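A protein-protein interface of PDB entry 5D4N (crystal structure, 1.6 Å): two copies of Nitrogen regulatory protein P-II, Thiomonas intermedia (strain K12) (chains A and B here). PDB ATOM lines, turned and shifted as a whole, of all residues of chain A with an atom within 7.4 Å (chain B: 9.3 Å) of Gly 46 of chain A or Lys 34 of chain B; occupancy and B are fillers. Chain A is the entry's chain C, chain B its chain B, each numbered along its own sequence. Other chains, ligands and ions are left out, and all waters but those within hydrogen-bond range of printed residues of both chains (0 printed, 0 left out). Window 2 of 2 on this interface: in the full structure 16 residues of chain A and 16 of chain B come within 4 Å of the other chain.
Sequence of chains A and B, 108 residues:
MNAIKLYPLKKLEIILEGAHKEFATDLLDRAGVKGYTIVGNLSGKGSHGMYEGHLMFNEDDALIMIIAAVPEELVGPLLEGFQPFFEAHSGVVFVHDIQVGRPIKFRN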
ATOM      1  N   GLY A  44       2.327  26.596  32.993  1.00  0.00           N
ATOM      2  CA  GLY A  44       2.762  26.768  31.622  1.00  0.00           C
ATOM      3  C   GLY A  44       1.701  26.388  30.623  1.00  0.00           C
ATOM      4  O   GLY A  44       0.613  25.940  30.995  1.00  0.00           O
ATOM      5  N   LYS A  45       2.030  26.580  29.348  1.00  0.00           N
ATOM      6  CA  LYS A  45       1.101  26.258  28.258  1.00  0.00           C
ATOM      7  C   LYS A  45       1.884  25.972  26.994  1.00  0.00           C
ATOM      8  O   LYS A  45       2.795  26.720  26.684  1.00  0.00           O
ATOM      9  CB  LYS A  45       0.150  27.443  28.031  1.00  0.00           C
ATOM     10  N   GLY A  46       1.497  24.930  26.251  1.00  0.00           N
ATOM     11  CA  GLY A  46       2.136  24.551  24.990  1.00  0.00           C
ATOM     12  C   GLY A  46       3.486  23.871  25.113  1.00  0.00           C
ATOM     13  O   GLY A  46       3.687  23.067  26.025  1.00  0.00           O
ATOM     14  N   SER A  47       4.430  24.181  24.188  1.00  0.00           N
ATOM     15  CA  SER A  47       5.809  23.664  24.218  1.00  0.00           C
ATOM     16  C   SER A  47       6.841  24.673  23.756  1.00  0.00           C
ATOM     17  O   SER A  47       6.662  25.321  22.736  1.00  0.00           O
ATOM     18  CB  SER A  47       5.956  22.350  23.464  1.00  0.00           C
ATOM     19  OG  SER A  47       7.204  21.769  23.809  1.00  0.00           O
ATOM     20  N   HIS A  48       7.923  24.824  24.527  1.00  0.00           N
ATOM     21  CA  HIS A  48       8.991  25.786  24.256  1.00  0.00           C
ATOM     22  C   HIS A  48       9.730  25.605  22.922  1.00  0.00           C
ATOM     23  O   HIS A  48      10.172  24.509  22.589  1.00  0.00           O
ATOM     24  CB  HIS A  48       9.949  25.800  25.422  1.00  0.00           C
ATOM     25  CG  HIS A  48       9.465  26.646  26.558  1.00  0.00           C
ATOM     26  ND1 HIS A  48       9.388  28.024  26.438  1.00  0.00           N
ATOM     27  CD2 HIS A  48       9.067  26.290  27.808  1.00  0.00           C
ATOM     28  CE1 HIS A  48       9.015  28.467  27.632  1.00  0.00           C
ATOM     29  NE2 HIS A  48       8.800  27.468  28.492  1.00  0.00           N
ATOM     30  N   MET A  56       2.939  18.450  25.328  1.00  0.00           N
ATOM     31  CA  MET A  56       2.573  19.837  25.648  1.00  0.00           C
ATOM     32  C   MET A  56       2.194  20.016  27.127  1.00  0.00           C
ATOM     33  O   MET A  56       1.783  19.056  27.784  1.00  0.00           O
ATOM     34  CB  MET A  56       1.402  20.311  24.754  1.00  0.00           C
ATOM     35  CG  MET A  56       1.830  21.083  23.510  1.00  0.00           C
ATOM     36  SD  MET A  56       0.403  21.663  22.535  1.00  0.00           S
ATOM     37  CE  MET A  56       1.082  23.085  21.776  1.00  0.00           C
ATOM     38  N   PHE A  57       2.322  21.252  27.643  1.00  0.00           N
ATOM     39  CA  PHE A  57       1.904  21.569  29.004  1.00  0.00           C
ATOM     40  C   PHE A  57       0.421  21.930  28.982  1.00  0.00           C
ATOM     41  O   PHE A  57      -0.024  22.711  28.129  1.00  0.00           O
ATOM     42  CB  PHE A  57       2.666  22.777  29.580  1.00  0.00           C
ATOM     43  CG  PHE A  57       4.172  22.724  29.648  1.00  0.00           C
ATOM     44  CD1 PHE A  57       4.818  21.699  30.332  1.00  0.00           C
ATOM     45  CD2 PHE A  57       4.944  23.757  29.125  1.00  0.00           C
ATOM     46  CE1 PHE A  57       6.210  21.669  30.426  1.00  0.00           C
ATOM     47  CE2 PHE A  57       6.339  23.725  29.213  1.00  0.00           C
ATOM     48  CZ  PHE A  57       6.962  22.687  29.874  1.00  0.00           C
ATOM     49  N   ASN A  58      -0.320  21.397  29.944  1.00  0.00           N
ATOM     50  CA  ASN A  58      -1.726  21.710  30.180  1.00  0.00           C
ATOM     51  C   ASN A  58      -1.701  22.827  31.228  1.00  0.00           C
ATOM     52  O   ASN A  58      -0.824  22.823  32.100  1.00  0.00           O
ATOM     53  CB  ASN A  58      -2.479  20.475  30.714  1.00  0.00           C
ATOM     54  N   GLU A  59      -2.640  23.786  31.135  1.00  0.00           N
ATOM     55  CA  GLU A  59      -2.742  24.942  32.042  1.00  0.00           C
ATOM     56  C   GLU A  59      -2.867  24.575  33.537  1.00  0.00           C
ATOM     57  O   GLU A  59      -2.448  25.360  34.396  1.00  0.00           O
ATOM     58  CB  GLU A  59      -3.898  25.857  31.608  1.00  0.00           C
ATOM     59  N   ASP A  61      -1.381  21.779  34.957  1.00  0.00           N
ATOM     60  CA  ASP A  61      -0.168  21.061  35.381  1.00  0.00           C
ATOM     61  C   ASP A  61       0.649  21.849  36.406  1.00  0.00           C
ATOM     62  O   ASP A  61       0.877  23.042  36.221  1.00  0.00           O
ATOM     63  CB  ASP A  61       0.750  20.784  34.175  1.00  0.00           C
ATOM     64  CG  ASP A  61       0.196  19.859  33.110  1.00  0.00           C
ATOM     65  OD1 ASP A  61      -0.668  19.013  33.443  1.00  0.00           O
ATOM     66  OD2 ASP A  61       0.677  19.933  31.961  1.00  0.00           O
ATOM     67  N   SER A  90       6.124  15.904  29.100  1.00  0.00           N
ATOM     68  CA  SER A  90       6.209  17.325  28.788  1.00  0.00           C
ATOM     69  C   SER A  90       7.448  17.906  29.470  1.00  0.00           C
ATOM     70  O   SER A  90       7.904  17.378  30.480  1.00  0.00           O
ATOM     71  CB  SER A  90       4.986  18.067  29.318  1.00  0.00           C
ATOM     72  OG  SER A  90       4.943  18.035  30.732  1.00  0.00           O
ATOM     73  N   GLY A  91       7.934  19.007  28.937  1.00  0.00           N
ATOM     74  CA  GLY A  91       9.067  19.699  29.531  1.00  0.00           C
ATOM     75  C   GLY A  91      10.196  19.999  28.582  1.00  0.00           C
ATOM     76  O   GLY A  91      10.176  19.573  27.424  1.00  0.00           O
ATOM     77  N   LEU B   9      18.809  29.124  20.541  1.00  0.00           N
ATOM     78  CA  LEU B   9      17.513  29.743  20.671  1.00  0.00           C
ATOM     79  C   LEU B   9      17.699  31.003  21.503  1.00  0.00           C
ATOM     80  O   LEU B   9      18.753  31.221  22.104  1.00  0.00           O
ATOM     81  CB  LEU B   9      16.510  28.814  21.386  1.00  0.00           C
ATOM     82  CG  LEU B   9      15.754  27.729  20.636  1.00  0.00           C
ATOM     83  CD1 LEU B   9      14.640  27.199  21.506  1.00  0.00           C
ATOM     84  CD2 LEU B   9      15.135  28.224  19.309  1.00  0.00           C
ATOM     85  N   THR B  25       0.406  36.865  27.453  1.00  0.00           N
ATOM     86  CA  THR B  25       0.267  35.528  26.876  1.00  0.00           C
ATOM     87  C   THR B  25      -0.457  35.561  25.535  1.00  0.00           C
ATOM     88  O   THR B  25      -0.076  34.807  24.636  1.00  0.00           O
ATOM     89  CB  THR B  25      -0.322  34.545  27.884  1.00  0.00           C
ATOM     90  OG1 THR B  25      -1.673  34.937  28.203  1.00  0.00           O
ATOM     91  CG2 THR B  25       0.559  34.400  29.138  1.00  0.00           C
ATOM     92  N   LEU B  27      -0.227  37.955  23.346  1.00  0.00           N
ATOM     93  CA  LEU B  27       0.754  38.473  22.409  1.00  0.00           C
ATOM     94  C   LEU B  27       1.729  37.363  22.026  1.00  0.00           C
ATOM     95  O   LEU B  27       2.095  37.268  20.854  1.00  0.00           O
ATOM     96  CB  LEU B  27       1.466  39.699  23.023  1.00  0.00           C
ATOM     97  CG  LEU B  27       2.622  40.349  22.253  1.00  0.00           C
ATOM     98  CD1 LEU B  27       2.224  40.719  20.827  1.00  0.00           C
ATOM     99  CD2 LEU B  27       3.067  41.629  22.970  1.00  0.00           C
ATOM    100  N   LEU B  28       2.129  36.512  22.993  1.00  0.00           N
ATOM    101  CA  LEU B  28       3.015  35.377  22.679  1.00  0.00           C
ATOM    102  C   LEU B  28       2.250  34.413  21.762  1.00  0.00           C
ATOM    103  O   LEU B  28       2.796  33.987  20.750  1.00  0.00           O
ATOM    104  CB  LEU B  28       3.465  34.649  23.937  1.00  0.00           C
ATOM    105  CG  LEU B  28       4.345  35.462  24.879  1.00  0.00           C
ATOM    106  CD1 LEU B  28       4.513  34.722  26.184  1.00  0.00           C
ATOM    107  CD2 LEU B  28       5.748  35.769  24.239  1.00  0.00           C
ATOM    108  N   ASP B  29       0.961  34.146  22.066  1.00  0.00           N
ATOM    109  CA  ASP B  29       0.124  33.245  21.254  1.00  0.00           C
ATOM    110  C   ASP B  29      -0.002  33.768  19.823  1.00  0.00           C
ATOM    111  O   ASP B  29       0.322  33.040  18.882  1.00  0.00           O
ATOM    112  CB  ASP B  29      -1.273  33.084  21.880  1.00  0.00           C
ATOM    113  CG  ASP B  29      -1.321  32.282  23.166  1.00  0.00           C
ATOM    114  OD1 ASP B  29      -0.314  31.599  23.486  1.00  0.00           O
ATOM    115  OD2 ASP B  29      -2.368  32.327  23.851  1.00  0.00           O
ATOM    116  N   ARG B  30      -0.368  35.060  19.671  1.00  0.00           N
ATOM    117  CA  ARG B  30      -0.543  35.708  18.365  1.00  0.00           C
ATOM    118  C   ARG B  30       0.744  35.792  17.540  1.00  0.00           C
ATOM    119  O   ARG B  30       0.657  35.748  16.320  1.00  0.00           O
ATOM    120  CB  ARG B  30      -1.221  37.076  18.498  1.00  0.00           C
ATOM    121  CG  ARG B  30      -2.687  36.980  18.911  1.00  0.00           C
ATOM    122  CD  ARG B  30      -3.359  38.336  18.885  1.00  0.00           C
ATOM    123  N   ALA B  31       1.932  35.829  18.192  1.00  0.00           N
ATOM    124  CA  ALA B  31       3.213  35.869  17.482  1.00  0.00           C
ATOM    125  C   ALA B  31       3.691  34.491  17.008  1.00  0.00           C
ATOM    126  O   ALA B  31       4.685  34.400  16.279  1.00  0.00           O
ATOM    127  CB  ALA B  31       4.278  36.524  18.346  1.00  0.00           C
ATOM    128  N   GLY B  32       3.025  33.437  17.454  1.00  0.00           N
ATOM    129  CA  GLY B  32       3.389  32.081  17.066  1.00  0.00           C
ATOM    130  C   GLY B  32       4.273  31.350  18.053  1.00  0.00           C
ATOM    131  O   GLY B  32       4.718  30.250  17.738  1.00  0.00           O
ATOM    132  N   VAL B  33       4.498  31.917  19.272  1.00  0.00           N
ATOM    133  CA  VAL B  33       5.308  31.285  20.329  1.00  0.00           C
ATOM    134  C   VAL B  33       4.617  29.983  20.692  1.00  0.00           C
ATOM    135  O   VAL B  33       3.410  29.972  20.904  1.00  0.00           O
ATOM    136  CB  VAL B  33       5.480  32.218  21.557  1.00  0.00           C
ATOM    137  CG1 VAL B  33       6.207  31.524  22.695  1.00  0.00           C
ATOM    138  CG2 VAL B  33       6.209  33.494  21.173  1.00  0.00           C
ATOM    139  N   LYS B  34       5.363  28.891  20.706  1.00  0.00           N
ATOM    140  CA  LYS B  34       4.767  27.578  20.911  1.00  0.00           C
ATOM    141  C   LYS B  34       4.474  27.163  22.331  1.00  0.00           C
ATOM    142  O   LYS B  34       3.659  26.267  22.552  1.00  0.00           O
ATOM    143  CB  LYS B  34       5.499  26.494  20.099  1.00  0.00           C
ATOM    144  CG  LYS B  34       5.359  26.682  18.594  1.00  0.00           C
ATOM    145  CD  LYS B  34       5.089  25.375  17.906  1.00  0.00           C
ATOM    146  CE  LYS B  34       4.809  25.542  16.431  1.00  0.00           C
ATOM    147  NZ  LYS B  34       3.400  25.944  16.157  1.00  0.00           N
ATOM    148  N   GLY B  35       5.123  27.812  23.286  1.00  0.00           N
ATOM    149  CA  GLY B  35       4.922  27.500  24.687  1.00  0.00           C
ATOM    150  C   GLY B  35       5.545  28.544  25.572  1.00  0.00           C
ATOM    151  O   GLY B  35       6.369  29.334  25.116  1.00  0.00           O
ATOM    152  N   TYR B  36       5.166  28.553  26.831  1.00  0.00           N
ATOM    153  CA  TYR B  36       5.750  29.487  27.785  1.00  0.00           C
ATOM    154  C   TYR B  36       5.573  28.908  29.175  1.00  0.00           C
ATOM    155  O   TYR B  36       4.742  27.999  29.359  1.00  0.00           O
ATOM    156  CB  TYR B  36       5.141  30.910  27.658  1.00  0.00           C
ATOM    157  CG  TYR B  36       3.636  30.949  27.783  1.00  0.00           C
ATOM    158  CD1 TYR B  36       3.015  30.826  29.025  1.00  0.00           C
ATOM    159  CD2 TYR B  36       2.829  31.126  26.666  1.00  0.00           C
ATOM    160  CE1 TYR B  36       1.623  30.853  29.150  1.00  0.00           C
ATOM    161  CE2 TYR B  36       1.442  31.180  26.779  1.00  0.00           C
ATOM    162  CZ  TYR B  36       0.839  31.014  28.020  1.00  0.00           C
ATOM    163  OH  TYR B  36      -0.539  31.057  28.121  1.00  0.00           O
ATOM    164  N   THR B  37       6.345  29.407  30.129  1.00  0.00           N
ATOM    165  CA  THR B  37       6.296  28.989  31.515  1.00  0.00           C
ATOM    166  C   THR B  37       6.167  30.258  32.355  1.00  0.00           C
ATOM    167  O   THR B  37       6.839  31.246  32.080  1.00  0.00           O
ATOM    168  CB  THR B  37       7.617  28.243  31.856  1.00  0.00           C
ATOM    169  OG1 THR B  37       7.638  27.063  31.058  1.00  0.00           O
ATOM    170  CG2 THR B  37       7.678  27.835  33.326  1.00  0.00           C
ATOM    171  N   ILE B  67       8.525  33.026  30.917  1.00  0.00           N
ATOM    172  CA  ILE B  67       9.753  32.538  30.269  1.00  0.00           C
ATOM    173  C   ILE B  67       9.309  31.954  28.931  1.00  0.00           C
ATOM    174  O   ILE B  67       8.429  31.076  28.896  1.00  0.00           O
ATOM    175  CB  ILE B  67      10.435  31.431  31.115  1.00  0.00           C
ATOM    176  CG1 ILE B  67      10.858  31.944  32.516  1.00  0.00           C
ATOM    177  CG2 ILE B  67      11.639  30.814  30.331  1.00  0.00           C
ATOM    178  CD1 ILE B  67      11.247  30.812  33.503  1.00  0.00           C
ATOM    179  N   ALA B  68       9.935  32.405  27.840  1.00  0.00           N
ATOM    180  CA  ALA B  68       9.617  31.855  26.514  1.00  0.00           C
ATOM    181  C   ALA B  68      10.912  31.635  25.752  1.00  0.00           C
ATOM    182  O   ALA B  68      11.703  32.555  25.672  1.00  0.00           O
ATOM    183  CB  ALA B  68       8.717  32.800  25.744  1.00  0.00           C
ATOM    184  N   ALA B  69      11.087  30.452  25.126  1.00  0.00           N
ATOM    185  CA  ALA B  69      12.278  30.195  24.314  1.00  0.00           C
ATOM    186  C   ALA B  69      11.783  30.240  22.893  1.00  0.00           C
ATOM    187  O   ALA B  69      10.833  29.543  22.523  1.00  0.00           O
ATOM    188  CB  ALA B  69      12.862  28.830  24.624  1.00  0.00           C
ATOM    189  N   VAL B  70      12.316  31.169  22.130  1.00  0.00           N
ATOM    190  CA  VAL B  70      11.844  31.405  20.777  1.00  0.00           C
ATOM    191  C   VAL B  70      12.997  31.413  19.778  1.00  0.00           C
ATOM    192  O   VAL B  70      14.115  31.763  20.132  1.00  0.00           O
ATOM    193  CB  VAL B  70      11.087  32.776  20.743  1.00  0.00           C
ATOM    194  CG1 VAL B  70       9.831  32.767  21.629  1.00  0.00           C
ATOM    195  CG2 VAL B  70      12.036  33.940  21.093  1.00  0.00           C
ATOM    196  N   PRO B  71      12.723  31.139  18.483  1.00  0.00           N
ATOM    197  CA  PRO B  71      13.772  31.326  17.463  1.00  0.00           C
ATOM    198  C   PRO B  71      14.163  32.807  17.418  1.00  0.00           C
ATOM    199  O   PRO B  71      13.318  33.670  17.672  1.00  0.00           O
ATOM    200  CB  PRO B  71      13.068  30.934  16.150  1.00  0.00           C
ATOM    201  CG  PRO B  71      11.828  30.219  16.545  1.00  0.00           C
ATOM    202  CD  PRO B  71      11.430  30.778  17.873  1.00  0.00           C
ATOM    203  N   LEU B  74      11.858  35.611  15.892  1.00  0.00           N
ATOM    204  CA  LEU B  74      10.634  36.066  16.563  1.00  0.00           C
ATOM    205  C   LEU B  74      10.901  37.143  17.621  1.00  0.00           C
ATOM    206  O   LEU B  74       9.959  37.802  18.071  1.00  0.00           O
ATOM    207  CB  LEU B  74       9.887  34.870  17.165  1.00  0.00           C
ATOM    208  CG  LEU B  74       8.439  34.978  17.596  1.00  0.00           C
ATOM    209  CD1 LEU B  74       7.616  35.980  16.753  1.00  0.00           C
ATOM    210  CD2 LEU B  74       7.833  33.594  17.651  1.00  0.00           C
ATOM    211  N   LEU B  78       8.279  40.285  18.609  1.00  0.00           N
ATOM    212  CA  LEU B  78       7.773  40.215  19.974  1.00  0.00           C
ATOM    213  C   LEU B  78       8.060  41.502  20.735  1.00  0.00           C
ATOM    214  O   LEU B  78       7.156  42.028  21.374  1.00  0.00           O
ATOM    215  CB  LEU B  78       8.343  39.012  20.737  1.00  0.00           C
ATOM    216  CG  LEU B  78       7.603  37.702  20.449  1.00  0.00           C
ATOM    217  CD1 LEU B  78       8.322  36.547  21.093  1.00  0.00           C
ATOM    218  CD2 LEU B  78       6.144  37.759  20.969  1.00  0.00           C
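O of Lys 34 of chain B is in hydrogen-bond range of N of Ser 47 of chain A (2.8 Å). The backbone carbonyl oxygen of Ser 47 of chain A is in hydrogen-bond range of the backbone NH of Gly 35 of chain B (3.0 Å). O of Lys 45 of chain A lies within hydrogen-bond range of N of Tyr 36 of chain B, at 3.0 Å. The side-chain hydroxyl of Thr 37 of chain B is in hydrogen-bond range of a ring nitrogen (NE2) of His 48 of chain A (2.8 Å). The backbone NH (N) of Ala 69 of chain B sits at hydrogen-bond distance from a ring nitrogen (ND1) of His 48 of chain A.
The backbone NH of Ile 67 of chain B sits at hydrogen-bond distance from the backbone carbonyl oxygen of Thr 37 of chain B, at 2.7 Å. The backbone carbonyl oxygen (O) of Gly 46 of chain A is in hydrogen-bond range of the backbone NH (N) of Phe 57 of chain A, 2.8 Å away.
CA of Gly 44 of chain A touches O of Tyr 36 of chain B (3.2 Å). Lys 45 of chain A touches Gly 35 of chain B (O to CA, 3.0 Å). CA of Gly 46 of chain A touches O of Lys 34 of chain B, at 3.3 Å. Gly 35 of chain B touches Gly 46 of chain A (CA to C, 3.9 Å). O of Gly 35 of chain B touches ND1 of His 48 of chain A (3.5 Å). CE1 of His 48 of chain A touches CA of Tyr 36 of chain B, 3.4 Å away. His 48 of chain A touches Ile 67 of chain B (CE1 to O, 3.0 Å). Ala 68 of chain B touches His 48 of chain A (CA to CE1, 3.6 Å).
Gly 46 of chain A touches just these residues of chain B: Lys 34 (3.3 Å) and Gly 35 (3.9 Å). Of chain A, only Gly 46 (3.3 Å) and Ser 47 (2.8 Å) come within 4 Å of Lys 34 of chain B. Of chain B, only Gly 35 and Tyr 36 come within 4 Å of Lys 45 of chain A. Ser 47 of chain A touches just these residues of chain B: Lys 34 and Gly 35. No residue of chain B comes within 4 Å of Met 56 of chain A. Printed residues of chain B within 4 Å of Gly 44 of chain A: Tyr 36. Of the printed residues of chain B, His 48 of chain A touches Gly 35 (3.5 Å), Tyr 36 (3.4 Å), Thr 37 (2.8 Å), Ile 67 (3.0 Å), Ala 68 (3.6 Å) and Ala 69 (3.2 Å). The nearest residue of chain A that does not touch Lys 34 of chain B is Met 56 of chain A (4.2 Å).
Of the 12 printed residues of chain A, 5 touch a printed residue of chain B. Among the printed residues, no Asp or Glu carboxylate lies within 4 Å of a Lys or Arg side-chain nitrogen of the other chain.
No position is printed for both chains.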
